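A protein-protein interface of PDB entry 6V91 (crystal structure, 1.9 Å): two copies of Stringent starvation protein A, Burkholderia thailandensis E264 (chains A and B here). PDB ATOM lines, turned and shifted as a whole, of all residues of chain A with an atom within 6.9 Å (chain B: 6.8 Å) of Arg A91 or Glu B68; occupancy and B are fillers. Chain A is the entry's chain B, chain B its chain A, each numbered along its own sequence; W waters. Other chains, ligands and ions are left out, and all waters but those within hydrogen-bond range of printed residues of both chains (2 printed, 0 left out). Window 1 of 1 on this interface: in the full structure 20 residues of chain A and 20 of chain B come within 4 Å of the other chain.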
ATOM      1  N   ILE A  65     -11.726  -3.123  -5.837  1.00  0.00           N
ATOM      2  CA  ILE A  65     -12.272  -4.288  -5.141  1.00  0.00           C
ATOM      3  C   ILE A  65     -11.690  -4.384  -3.737  1.00  0.00           C
ATOM      4  O   ILE A  65     -12.420  -4.558  -2.747  1.00  0.00           O
ATOM      5  CB  ILE A  65     -11.992  -5.567  -5.952  1.00  0.00           C
ATOM      6  CG1 ILE A  65     -12.785  -5.568  -7.267  1.00  0.00           C
ATOM      7  CG2 ILE A  65     -12.259  -6.827  -5.112  1.00  0.00           C
ATOM      8  CD1 ILE A  65     -14.296  -5.829  -7.111  1.00  0.00           C
ATOM      9  N   GLU A  68     -13.009  -1.399  -1.600  1.00  0.00           N
ATOM     10  CA  GLU A  68     -14.408  -1.585  -1.249  1.00  0.00           C
ATOM     11  C   GLU A  68     -14.557  -2.602  -0.124  1.00  0.00           C
ATOM     12  O   GLU A  68     -15.380  -2.424   0.785  1.00  0.00           O
ATOM     13  CB  GLU A  68     -15.187  -2.012  -2.489  1.00  0.00           C
ATOM     14  CG  GLU A  68     -16.669  -2.164  -2.293  1.00  0.00           C
ATOM     15  CD  GLU A  68     -17.381  -2.371  -3.629  1.00  0.00           C
ATOM     16  OE1 GLU A  68     -16.853  -3.129  -4.483  1.00  0.00           O
ATOM     17  OE2 GLU A  68     -18.451  -1.756  -3.832  1.00  0.00           O
ATOM     18  N   GLU A  72     -15.926  -1.919   3.873  1.00  0.00           N
ATOM     19  CA  GLU A  72     -17.023  -2.650   4.503  1.00  0.00           C
ATOM     20  C   GLU A  72     -16.582  -3.402   5.761  1.00  0.00           C
ATOM     21  O   GLU A  72     -17.361  -3.505   6.717  1.00  0.00           O
ATOM     22  CB  GLU A  72     -17.664  -3.605   3.484  1.00  0.00           C
ATOM     23  CG  GLU A  72     -18.335  -2.849   2.317  1.00  0.00           C
ATOM     24  CD  GLU A  72     -19.040  -3.751   1.282  1.00  0.00           C
ATOM     25  OE1 GLU A  72     -19.129  -4.991   1.482  1.00  0.00           O
ATOM     26  OE2 GLU A  72     -19.509  -3.197   0.260  1.00  0.00           O
ATOM     27  N   MET A  80     -17.750   5.802   1.450  1.00  0.00           N
ATOM     28  CA  MET A  80     -18.863   5.875   0.513  1.00  0.00           C
ATOM     29  C   MET A  80     -20.097   6.374   1.252  1.00  0.00           C
ATOM     30  O   MET A  80     -20.222   6.160   2.462  1.00  0.00           O
ATOM     31  CB  MET A  80     -19.157   4.509  -0.130  1.00  0.00           C
ATOM     32  CG  MET A  80     -18.071   4.045  -1.097  1.00  0.00           C
ATOM     33  SD  MET A  80     -17.797   5.193  -2.480  1.00  0.00           S
ATOM     34  CE  MET A  80     -18.946   4.523  -3.692  1.00  0.00           C
ATOM     35  N   PRO A  81     -21.003   7.064   0.563  1.00  0.00           N
ATOM     36  CA  PRO A  81     -22.227   7.527   1.230  1.00  0.00           C
ATOM     37  C   PRO A  81     -22.960   6.369   1.886  1.00  0.00           C
ATOM     38  O   PRO A  81     -22.966   5.248   1.373  1.00  0.00           O
ATOM     39  CB  PRO A  81     -23.049   8.126   0.087  1.00  0.00           C
ATOM     40  CG  PRO A  81     -22.056   8.516  -0.953  1.00  0.00           C
ATOM     41  CD  PRO A  81     -20.882   7.583  -0.810  1.00  0.00           C
ATOM     42  N   GLN A  86     -27.245   7.886  -2.976  1.00  0.00           N
ATOM     43  CA  GLN A  86     -25.972   8.584  -3.109  1.00  0.00           C
ATOM     44  C   GLN A  86     -24.839   7.597  -3.361  1.00  0.00           C
ATOM     45  O   GLN A  86     -23.908   7.880  -4.125  1.00  0.00           O
ATOM     46  CB  GLN A  86     -25.687   9.420  -1.851  1.00  0.00           C
ATOM     47  CG  GLN A  86     -26.720  10.511  -1.523  1.00  0.00           C
ATOM     48  CD  GLN A  86     -26.319  11.379  -0.324  1.00  0.00           C
ATOM     49  OE1 GLN A  86     -25.244  11.208   0.260  1.00  0.00           O
ATOM     50  NE2 GLN A  86     -27.187  12.318   0.040  1.00  0.00           N
ATOM     51  N   ARG A  87     -24.904   6.430  -2.723  1.00  0.00           N
ATOM     52  CA  ARG A  87     -23.855   5.436  -2.899  1.00  0.00           C
ATOM     53  C   ARG A  87     -23.879   4.842  -4.307  1.00  0.00           C
ATOM     54  O   ARG A  87     -22.822   4.621  -4.912  1.00  0.00           O
ATOM     55  CB  ARG A  87     -23.989   4.340  -1.843  1.00  0.00           C
ATOM     56  CG  ARG A  87     -22.988   3.201  -2.022  1.00  0.00           C
ATOM     57  CD  ARG A  87     -22.869   2.314  -0.782  1.00  0.00           C
ATOM     58  NE  ARG A  87     -24.131   1.682  -0.400  1.00  0.00           N
ATOM     59  CZ  ARG A  87     -24.891   2.106   0.605  1.00  0.00           C
ATOM     60  NH1 ARG A  87     -26.019   1.493   0.901  1.00  0.00           N
ATOM     61  NH2 ARG A  87     -24.520   3.155   1.316  1.00  0.00           N
ATOM     62  N   ALA A  88     -25.071   4.569  -4.841  1.00  0.00           N
ATOM     63  CA  ALA A  88     -25.170   4.118  -6.225  1.00  0.00           C
ATOM     64  C   ALA A  88     -24.605   5.162  -7.187  1.00  0.00           C
ATOM     65  O   ALA A  88     -23.854   4.826  -8.112  1.00  0.00           O
ATOM     66  CB  ALA A  88     -26.628   3.784  -6.570  1.00  0.00           C
ATOM     67  N   ARG A  89     -24.943   6.440  -6.983  1.00  0.00           N
ATOM     68  CA  ARG A  89     -24.371   7.490  -7.823  1.00  0.00           C
ATOM     69  C   ARG A  89     -22.847   7.509  -7.724  1.00  0.00           C
ATOM     70  O   ARG A  89     -22.145   7.678  -8.735  1.00  0.00           O
ATOM     71  CB  ARG A  89     -24.937   8.855  -7.430  1.00  0.00           C
ATOM     72  CG  ARG A  89     -26.411   9.107  -7.818  1.00  0.00           C
ATOM     73  CD  ARG A  89     -26.679  10.615  -7.818  1.00  0.00           C
ATOM     74  NE  ARG A  89     -28.070  10.965  -8.120  1.00  0.00           N
ATOM     75  CZ  ARG A  89     -28.979  11.251  -7.196  1.00  0.00           C
ATOM     76  NH1 ARG A  89     -30.219  11.572  -7.541  1.00  0.00           N
ATOM     77  NH2 ARG A  89     -28.643  11.225  -5.915  1.00  0.00           N
ATOM     78  N   ALA A  90     -22.311   7.337  -6.512  1.00  0.00           N
ATOM     79  CA  ALA A  90     -20.861   7.391  -6.352  1.00  0.00           C
ATOM     80  C   ALA A  90     -20.186   6.177  -6.990  1.00  0.00           C
ATOM     81  O   ALA A  90     -19.094   6.304  -7.558  1.00  0.00           O
ATOM     82  CB  ALA A  90     -20.493   7.508  -4.868  1.00  0.00           C
ATOM     83  N   ARG A  91     -20.808   4.995  -6.900  1.00  0.00           N
ATOM     84  CA  ARG A  91     -20.244   3.819  -7.558  1.00  0.00           C
ATOM     85  C   ARG A  91     -20.182   4.016  -9.068  1.00  0.00           C
ATOM     86  O   ARG A  91     -19.208   3.598  -9.717  1.00  0.00           O
ATOM     87  CB  ARG A  91     -21.056   2.565  -7.211  1.00  0.00           C
ATOM     88  CG  ARG A  91     -21.014   2.174  -5.723  1.00  0.00           C
ATOM     89  CD  ARG A  91     -21.747   0.844  -5.437  1.00  0.00           C
ATOM     90  NE  ARG A  91     -20.842  -0.294  -5.572  1.00  0.00           N
ATOM     91  CZ  ARG A  91     -21.016  -1.317  -6.401  1.00  0.00           C
ATOM     92  NH1 ARG A  91     -22.106  -1.381  -7.175  1.00  0.00           N
ATOM     93  NH2 ARG A  91     -20.098  -2.286  -6.433  1.00  0.00           N
ATOM     94  N   LEU A  92     -21.208   4.656  -9.641  1.00  0.00           N
ATOM     95  CA  LEU A  92     -21.221   4.961 -11.068  1.00  0.00           C
ATOM     96  C   LEU A  92     -20.146   5.981 -11.420  1.00  0.00           C
ATOM     97  O   LEU A  92     -19.455   5.836 -12.438  1.00  0.00           O
ATOM     98  CB  LEU A  92     -22.608   5.462 -11.477  1.00  0.00           C
ATOM     99  CG  LEU A  92     -22.860   5.765 -12.959  1.00  0.00           C
ATOM    100  CD1 LEU A  92     -22.342   4.646 -13.838  1.00  0.00           C
ATOM    101  CD2 LEU A  92     -24.325   5.939 -13.200  1.00  0.00           C
ATOM    102  N   PHE A  93     -19.978   7.016 -10.588  1.00  0.00           N
ATOM    103  CA  PHE A  93     -18.905   7.973 -10.839  1.00  0.00           C
ATOM    104  C   PHE A  93     -17.538   7.291 -10.792  1.00  0.00           C
ATOM    105  O   PHE A  93     -16.672   7.573 -11.632  1.00  0.00           O
ATOM    106  CB  PHE A  93     -18.987   9.133  -9.842  1.00  0.00           C
ATOM    107  CG  PHE A  93     -18.671  10.496 -10.439  1.00  0.00           C
ATOM    108  CD1 PHE A  93     -19.615  11.189 -11.186  1.00  0.00           C
ATOM    109  CD2 PHE A  93     -17.444  11.088 -10.232  1.00  0.00           C
ATOM    110  CE1 PHE A  93     -19.331  12.443 -11.724  1.00  0.00           C
ATOM    111  CE2 PHE A  93     -17.153  12.346 -10.771  1.00  0.00           C
ATOM    112  CZ  PHE A  93     -18.094  13.019 -11.517  1.00  0.00           C
ATOM    113  N   LEU A  94     -17.323   6.378  -9.835  1.00  0.00           N
ATOM    114  CA  LEU A  94     -16.045   5.669  -9.762  1.00  0.00           C
ATOM    115  C   LEU A  94     -15.818   4.820 -10.997  1.00  0.00           C
ATOM    116  O   LEU A  94     -14.703   4.759 -11.533  1.00  0.00           O
ATOM    117  CB  LEU A  94     -15.993   4.766  -8.536  1.00  0.00           C
ATOM    118  CG  LEU A  94     -15.656   5.296  -7.156  1.00  0.00           C
ATOM    119  CD1 LEU A  94     -15.961   4.184  -6.165  1.00  0.00           C
ATOM    120  CD2 LEU A  94     -14.189   5.723  -7.075  1.00  0.00           C
ATOM    121  N   LEU A  95     -16.860   4.119 -11.436  1.00  0.00           N
ATOM    122  CA  LEU A  95     -16.738   3.281 -12.619  1.00  0.00           C
ATOM    123  C   LEU A  95     -16.373   4.119 -13.833  1.00  0.00           C
ATOM    124  O   LEU A  95     -15.499   3.737 -14.621  1.00  0.00           O
ATOM    125  CB  LEU A  95     -18.044   2.519 -12.837  1.00  0.00           C
ATOM    126  CG  LEU A  95     -18.007   1.403 -13.884  1.00  0.00           C
ATOM    127  CD1 LEU A  95     -16.924   0.369 -13.574  1.00  0.00           C
ATOM    128  CD2 LEU A  95     -19.355   0.739 -13.917  1.00  0.00           C
ATOM    129  N   ASN A  96     -16.987   5.296 -13.971  1.00  0.00           N
ATOM    130  CA  ASN A  96     -16.671   6.151 -15.109  1.00  0.00           C
ATOM    131  C   ASN A  96     -15.246   6.692 -15.036  1.00  0.00           C
ATOM    132  O   ASN A  96     -14.605   6.896 -16.074  1.00  0.00           O
ATOM    133  CB  ASN A  96     -17.683   7.299 -15.202  1.00  0.00           C
ATOM    134  CG  ASN A  96     -19.041   6.841 -15.731  1.00  0.00           C
ATOM    135  OD1 ASN A  96     -19.155   5.764 -16.321  1.00  0.00           O
ATOM    136  ND2 ASN A  96     -20.068   7.670 -15.542  1.00  0.00           N
ATOM    137  N   LEU A 152     -13.921   8.415  -4.016  1.00  0.00           N
ATOM    138  CA  LEU A 152     -13.619   9.137  -5.249  1.00  0.00           C
ATOM    139  C   LEU A 152     -12.305   9.912  -5.110  1.00  0.00           C
ATOM    140  O   LEU A 152     -11.467   9.900  -6.020  1.00  0.00           O
ATOM    141  CB  LEU A 152     -14.773  10.069  -5.619  1.00  0.00           C
ATOM    142  CG  LEU A 152     -15.970   9.414  -6.343  1.00  0.00           C
ATOM    143  CD1 LEU A 152     -16.651   8.379  -5.472  1.00  0.00           C
ATOM    144  CD2 LEU A 152     -16.995  10.455  -6.763  1.00  0.00           C
ATOM    145  N   VAL B  19     -33.257  -9.462 -12.978  1.00  0.00           N
ATOM    146  CA  VAL B  19     -33.243  -9.059 -11.573  1.00  0.00           C
ATOM    147  C   VAL B  19     -34.618  -8.573 -11.141  1.00  0.00           C
ATOM    148  O   VAL B  19     -35.111  -8.914 -10.056  1.00  0.00           O
ATOM    149  CB  VAL B  19     -32.181  -7.973 -11.352  1.00  0.00           C
ATOM    150  CG1 VAL B  19     -32.390  -7.288  -9.961  1.00  0.00           C
ATOM    151  CG2 VAL B  19     -30.789  -8.579 -11.467  1.00  0.00           C
ATOM    152  N   SER B  63     -25.302  -1.979 -16.333  1.00  0.00           N
ATOM    153  CA  SER B  63     -26.214  -2.994 -15.804  1.00  0.00           C
ATOM    154  C   SER B  63     -25.803  -3.451 -14.412  1.00  0.00           C
ATOM    155  O   SER B  63     -26.661  -3.638 -13.548  1.00  0.00           O
ATOM    156  CB  SER B  63     -26.324  -4.190 -16.760  1.00  0.00           C
ATOM    157  OG  SER B  63     -25.046  -4.768 -17.012  1.00  0.00           O
ATOM    158  N   ASN B  64     -24.496  -3.622 -14.157  1.00  0.00           N
ATOM    159  CA  ASN B  64     -24.099  -4.089 -12.832  1.00  0.00           C
ATOM    160  C   ASN B  64     -24.329  -3.028 -11.751  1.00  0.00           C
ATOM    161  O   ASN B  64     -24.655  -3.378 -10.613  1.00  0.00           O
ATOM    162  CB  ASN B  64     -22.634  -4.540 -12.852  1.00  0.00           C
ATOM    163  CG  ASN B  64     -22.469  -5.934 -13.483  1.00  0.00           C
ATOM    164  OD1 ASN B  64     -23.450  -6.642 -13.710  1.00  0.00           O
ATOM    165  ND2 ASN B  64     -21.239  -6.326 -13.744  1.00  0.00           N
ATOM    166  N   ILE B  65     -24.166  -1.744 -12.079  1.00  0.00           N
ATOM    167  CA  ILE B  65     -24.512  -0.677 -11.137  1.00  0.00           C
ATOM    168  C   ILE B  65     -26.008  -0.704 -10.830  1.00  0.00           C
ATOM    169  O   ILE B  65     -26.434  -0.618  -9.668  1.00  0.00           O
ATOM    170  CB  ILE B  65     -24.078   0.686 -11.703  1.00  0.00           C
ATOM    171  CG1 ILE B  65     -22.547   0.776 -11.830  1.00  0.00           C
ATOM    172  CG2 ILE B  65     -24.619   1.829 -10.846  1.00  0.00           C
ATOM    173  CD1 ILE B  65     -21.818   1.035 -10.510  1.00  0.00           C
ATOM    174  N   ILE B  66     -26.831  -0.808 -11.868  1.00  0.00           N
ATOM    175  CA  ILE B  66     -28.276  -0.811 -11.659  1.00  0.00           C
ATOM    176  C   ILE B  66     -28.675  -1.970 -10.755  1.00  0.00           C
ATOM    177  O   ILE B  66     -29.436  -1.807  -9.788  1.00  0.00           O
ATOM    178  CB  ILE B  66     -29.004  -0.899 -13.012  1.00  0.00           C
ATOM    179  CG1 ILE B  66     -28.885   0.428 -13.775  1.00  0.00           C
ATOM    180  CG2 ILE B  66     -30.474  -1.325 -12.771  1.00  0.00           C
ATOM    181  CD1 ILE B  66     -29.215   0.272 -15.305  1.00  0.00           C
ATOM    182  N   ASN B  67     -28.148  -3.164 -11.056  1.00  0.00           N
ATOM    183  CA  ASN B  67     -28.551  -4.371 -10.347  1.00  0.00           C
ATOM    184  C   ASN B  67     -28.059  -4.381  -8.910  1.00  0.00           C
ATOM    185  O   ASN B  67     -28.760  -4.897  -8.034  1.00  0.00           O
ATOM    186  CB  ASN B  67     -28.043  -5.608 -11.108  1.00  0.00           C
ATOM    187  CG  ASN B  67     -28.809  -5.830 -12.399  1.00  0.00           C
ATOM    188  OD1 ASN B  67     -29.910  -5.308 -12.558  1.00  0.00           O
ATOM    189  ND2 ASN B  67     -28.244  -6.606 -13.320  1.00  0.00           N
ATOM    190  N   GLU B  68     -26.873  -3.819  -8.640  1.00  0.00           N
ATOM    191  CA  GLU B  68     -26.436  -3.697  -7.260  1.00  0.00           C
ATOM    192  C   GLU B  68     -27.350  -2.747  -6.493  1.00  0.00           C
ATOM    193  O   GLU B  68     -27.648  -2.974  -5.318  1.00  0.00           O
ATOM    194  CB  GLU B  68     -24.983  -3.202  -7.193  1.00  0.00           C
ATOM    195  CG  GLU B  68     -23.932  -4.294  -7.395  1.00  0.00           C
ATOM    196  CD  GLU B  68     -22.891  -4.321  -6.271  1.00  0.00           C
ATOM    197  OE1 GLU B  68     -21.809  -4.934  -6.449  1.00  0.00           O
ATOM    198  OE2 GLU B  68     -23.161  -3.728  -5.207  1.00  0.00           O
ATOM    199  N   TYR B  69     -27.785  -1.664  -7.139  1.00  0.00           N
ATOM    200  CA  TYR B  69     -28.702  -0.729  -6.483  1.00  0.00           C
ATOM    201  C   TYR B  69     -30.023  -1.416  -6.138  1.00  0.00           C
ATOM    202  O   TYR B  69     -30.536  -1.286  -5.016  1.00  0.00           O
ATOM    203  CB  TYR B  69     -28.953   0.481  -7.389  1.00  0.00           C
ATOM    204  CG  TYR B  69     -30.063   1.378  -6.845  1.00  0.00           C
ATOM    205  CD1 TYR B  69     -29.875   2.113  -5.693  1.00  0.00           C
ATOM    206  CD2 TYR B  69     -31.304   1.438  -7.474  1.00  0.00           C
ATOM    207  CE1 TYR B  69     -30.881   2.916  -5.172  1.00  0.00           C
ATOM    208  CE2 TYR B  69     -32.319   2.235  -6.970  1.00  0.00           C
ATOM    209  CZ  TYR B  69     -32.105   2.964  -5.822  1.00  0.00           C
ATOM    210  OH  TYR B  69     -33.107   3.757  -5.316  1.00  0.00           O
ATOM    211  N   ILE B  70     -30.590  -2.139  -7.104  1.00  0.00           N
ATOM    212  CA  ILE B  70     -31.860  -2.836  -6.893  1.00  0.00           C
ATOM    213  C   ILE B  70     -31.711  -3.903  -5.817  1.00  0.00           C
ATOM    214  O   ILE B  70     -32.576  -4.054  -4.947  1.00  0.00           O
ATOM    215  CB  ILE B  70     -32.354  -3.441  -8.223  1.00  0.00           C
ATOM    216  CG1 ILE B  70     -32.740  -2.343  -9.216  1.00  0.00           C
ATOM    217  CG2 ILE B  70     -33.563  -4.368  -8.026  1.00  0.00           C
ATOM    218  CD1 ILE B  70     -32.888  -2.905 -10.650  1.00  0.00           C
ATOM    219  N   ASP B  71     -30.600  -4.649  -5.845  1.00  0.00           N
ATOM    220  CA  ASP B  71     -30.412  -5.716  -4.864  1.00  0.00           C
ATOM    221  C   ASP B  71     -30.337  -5.166  -3.444  1.00  0.00           C
ATOM    222  O   ASP B  71     -30.868  -5.779  -2.510  1.00  0.00           O
ATOM    223  CB  ASP B  71     -29.161  -6.524  -5.203  1.00  0.00           C
ATOM    224  CG  ASP B  71     -29.099  -7.841  -4.449  1.00  0.00           C
ATOM    225  OD1 ASP B  71     -30.080  -8.622  -4.517  1.00  0.00           O
ATOM    226  OD2 ASP B  71     -28.063  -8.107  -3.807  1.00  0.00           O
ATOM    227  N   GLU B  72     -29.726  -3.991  -3.254  1.00  0.00           N
ATOM    228  CA  GLU B  72     -29.676  -3.409  -1.915  1.00  0.00           C
ATOM    229  C   GLU B  72     -31.043  -2.878  -1.495  1.00  0.00           C
ATOM    230  O   GLU B  72     -31.436  -2.993  -0.328  1.00  0.00           O
ATOM    231  CB  GLU B  72     -28.620  -2.299  -1.863  1.00  0.00           C
ATOM    232  CG  GLU B  72     -27.195  -2.813  -2.062  1.00  0.00           C
ATOM    233  CD  GLU B  72     -26.125  -1.719  -2.182  1.00  0.00           C
ATOM    234  OE1 GLU B  72     -26.406  -0.557  -1.820  1.00  0.00           O
ATOM    235  OE2 GLU B  72     -24.994  -2.026  -2.635  1.00  0.00           O
ATOM    236  N   ARG B  73     -31.776  -2.282  -2.427  1.00  0.00           N
ATOM    237  CA  ARG B  73     -33.067  -1.712  -2.059  1.00  0.00           C
ATOM    238  C   ARG B  73     -34.116  -2.799  -1.847  1.00  0.00           C
ATOM    239  O   ARG B  73     -35.016  -2.635  -1.018  1.00  0.00           O
ATOM    240  CB  ARG B  73     -33.540  -0.740  -3.136  1.00  0.00           C
ATOM    241  CG  ARG B  73     -32.771   0.560  -3.184  1.00  0.00           C
ATOM    242  CD  ARG B  73     -33.572   1.700  -2.555  1.00  0.00           C
ATOM    243  NE  ARG B  73     -34.718   2.108  -3.372  1.00  0.00           N
ATOM    244  CZ  ARG B  73     -35.974   1.738  -3.144  1.00  0.00           C
ATOM    245  NH1 ARG B  73     -36.949   2.164  -3.937  1.00  0.00           N
ATOM    246  NH2 ARG B  73     -36.258   0.943  -2.121  1.00  0.00           N
ATOM    247  N   MET B  80     -26.483 -10.481  -4.282  1.00  0.00           N
ATOM    248  CA  MET B  80     -25.096 -10.346  -3.831  1.00  0.00           C
ATOM    249  C   MET B  80     -24.977 -10.949  -2.446  1.00  0.00           C
ATOM    250  O   MET B  80     -25.817 -10.658  -1.589  1.00  0.00           O
ATOM    251  CB  MET B  80     -24.679  -8.881  -3.783  1.00  0.00           C
ATOM    252  CG  MET B  80     -24.802  -8.133  -5.107  1.00  0.00           C
ATOM    253  SD  MET B  80     -23.527  -8.629  -6.304  1.00  0.00           S
ATOM    254  CE  MET B  80     -22.108  -8.816  -5.225  1.00  0.00           C
ATOM    255  N   ARG B  87     -18.976 -11.456  -0.588  1.00  0.00           N
ATOM    256  CA  ARG B  87     -19.416 -10.393  -1.491  1.00  0.00           C
ATOM    257  C   ARG B  87     -18.243  -9.854  -2.306  1.00  0.00           C
ATOM    258  O   ARG B  87     -18.355  -9.667  -3.529  1.00  0.00           O
ATOM    259  CB  ARG B  87     -20.108  -9.273  -0.696  1.00  0.00           C
ATOM    260  CG  ARG B  87     -20.701  -8.147  -1.563  1.00  0.00           C
ATOM    261  CD  ARG B  87     -21.705  -7.255  -0.808  1.00  0.00           C
ATOM    262  NE  ARG B  87     -21.109  -6.686   0.399  1.00  0.00           N
ATOM    263  CZ  ARG B  87     -21.410  -7.067   1.639  1.00  0.00           C
ATOM    264  NH1 ARG B  87     -22.322  -8.014   1.845  1.00  0.00           N
ATOM    265  NH2 ARG B  87     -20.807  -6.493   2.675  1.00  0.00           N
ATOM    266  N   ARG B  91     -17.845  -9.859  -6.275  1.00  0.00           N
ATOM    267  CA  ARG B  91     -17.611  -8.644  -7.049  1.00  0.00           C
ATOM    268  C   ARG B  91     -16.392  -8.800  -7.942  1.00  0.00           C
ATOM    269  O   ARG B  91     -16.364  -8.280  -9.064  1.00  0.00           O
ATOM    270  CB  ARG B  91     -17.452  -7.436  -6.128  1.00  0.00           C
ATOM    271  CG  ARG B  91     -18.790  -6.916  -5.583  1.00  0.00           C
ATOM    272  CD  ARG B  91     -18.617  -5.847  -4.505  1.00  0.00           C
ATOM    273  NE  ARG B  91     -19.930  -5.288  -4.200  1.00  0.00           N
ATOM    274  CZ  ARG B  91     -20.255  -4.652  -3.084  1.00  0.00           C
ATOM    275  NH1 ARG B  91     -19.354  -4.472  -2.111  1.00  0.00           N
ATOM    276  NH2 ARG B  91     -21.494  -4.187  -2.951  1.00  0.00           N
ATOM    277  N   LEU B  94     -17.540 -10.841 -10.950  1.00  0.00           N
ATOM    278  CA  LEU B  94     -18.272  -9.967 -11.864  1.00  0.00           C
ATOM    279  C   LEU B  94     -17.332  -9.080 -12.654  1.00  0.00           C
ATOM    280  O   LEU B  94     -17.533  -8.859 -13.854  1.00  0.00           O
ATOM    281  CB  LEU B  94     -19.262  -9.090 -11.106  1.00  0.00           C
ATOM    282  CG  LEU B  94     -20.440  -9.843 -10.531  1.00  0.00           C
ATOM    283  CD1 LEU B  94     -21.228  -8.901  -9.638  1.00  0.00           C
ATOM    284  CD2 LEU B  94     -21.277 -10.354 -11.690  1.00  0.00           C
ATOM    285  N   MET B 151     -25.958 -12.945  -8.331  1.00  0.00           N
ATOM    286  CA  MET B 151     -25.688 -11.989  -9.394  1.00  0.00           C
ATOM    287  C   MET B 151     -24.715 -12.538 -10.435  1.00  0.00           C
ATOM    288  O   MET B 151     -24.744 -12.102 -11.587  1.00  0.00           O
ATOM    289  CB  MET B 151     -25.132 -10.699  -8.792  1.00  0.00           C
ATOM    290  CG  MET B 151     -25.331  -9.496  -9.684  1.00  0.00           C
ATOM    291  SD  MET B 151     -27.077  -9.041  -9.868  1.00  0.00           S
ATOM    292  CE  MET B 151     -27.293  -8.062  -8.381  1.00  0.00           C
HETATM  293  O   HOH W   1     -24.611   0.440  -7.537  1.00  0.00           O
HETATM  294  O   HOH W   2     -22.384  -3.090  -0.304  1.00  0.00           O
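OE1 of Glu B68 lies within salt-bridge range of NH2 of Arg A91, at 3.2 Å.
OE1 of Glu B72 lies within salt-bridge range of NH1 of Arg A87, 3.4 Å away.
OE1 of Glu A72 is in salt-bridge range of NH2 of Arg B87 (2.5 Å).
The guanidinium group of Arg B91 is in salt-bridge range of the side-chain carboxylate of Glu A68 (3.3 Å).
The guanidinium group (NH1) of Arg B91 is in salt-bridge range of the side-chain carboxylate (OE2) of Glu A72 (2.7 Å).
Glu A68 touches Arg B91, and with the chains exchanged Arg A91 touches Glu B68.
Glu A72 touches Arg B87, and with the chains exchanged Arg A87 touches Glu B72.
Glu A72 touches Arg B91, but with the chains exchanged Arg A91 does not touch Glu B72 (5.2 Å).
Arg B91 touches its own counterpart, Arg A91.
7 positions are printed for both chains.
Of the 11 pairs that touch across the chains among the printed residues, 7 have their exchanged pair printed and touching as well.
Of the printed residues of chain B, Arg A91 touches Ile B65, Glu B68 and Arg B91.
Of the printed residues of chain A, Glu B68 touches Arg A91 (3.2 Å).
Printed residues of chain B within 4 Å of Leu A92: Ile B65 (3.8 Å).
Printed residues of chain B within 4 Å of Arg A87: Glu B72.
Of the printed residues of chain B, Ile A65 touches Arg B91 (3.7 Å).
Printed residues of chain B within 4 Å of Glu A68: Arg B91 (3.2 Å).
Of the printed residues of chain A, Arg B87 touches Glu A72 (2.5 Å).
Gln A86 touches none of the printed residues of chain B.
The nearest printed residue of chain B that does not touch Arg A91 is Asn B64 (4.7 Å).
The nearest printed residue of chain A that does not touch Glu B68 is Glu A68 (5.3 Å).
The nearest printed residue of chain B that does not touch Ala A88 is Ile B65 (4.1 Å).
Arg B91 touches Ile A65 (CB to CD1, 3.7 Å).
Ala A88 touches Tyr B69.
CD1 of Ile B65 touches C of Arg A91, 3.7 Å away.
Arg A91 touches Arg B91 (NH2 to NE, 3.7 Å).
Leu A92 touches Ile B65 (N to CD1, 3.8 Å).
Leu A95 touches Ile B65.
Hydrophobic or aromatic side chains of chain B within 4 Å of the printed part of chain A: Ile B65 and Tyr B69.
Of the 17 printed residues of chain A, 8 touch a printed residue of chain B.
Hydrophobic or aromatic side chains of chain A within 4 Å of the printed part of chain B: Ile A65, Ala A88 and Leu A95.
Water W2 lies within hydrogen-bond range of OE2 of Glu A72 (2.9 Å) and NH2 of Arg B91 (3.0 Å).
Water W1 bridges O of Ile B65 and NH1 of Arg A91.
OE2 of Glu B68 lies within salt-bridge range of NH2 of Arg B91 (2.8 Å).
The guanidinium group (NE) of Arg B73 is in hydrogen-bond range of the side-chain hydroxyl (OH) of Tyr B69, 3.0 Å away.
The side-chain carboxylate of Glu A68 is in salt-bridge range of the guanidinium group of Arg A91 (3.1 Å).
O of Pro A81 is in hydrogen-bond range of NH2 of Arg A87, 2.6 Å away.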
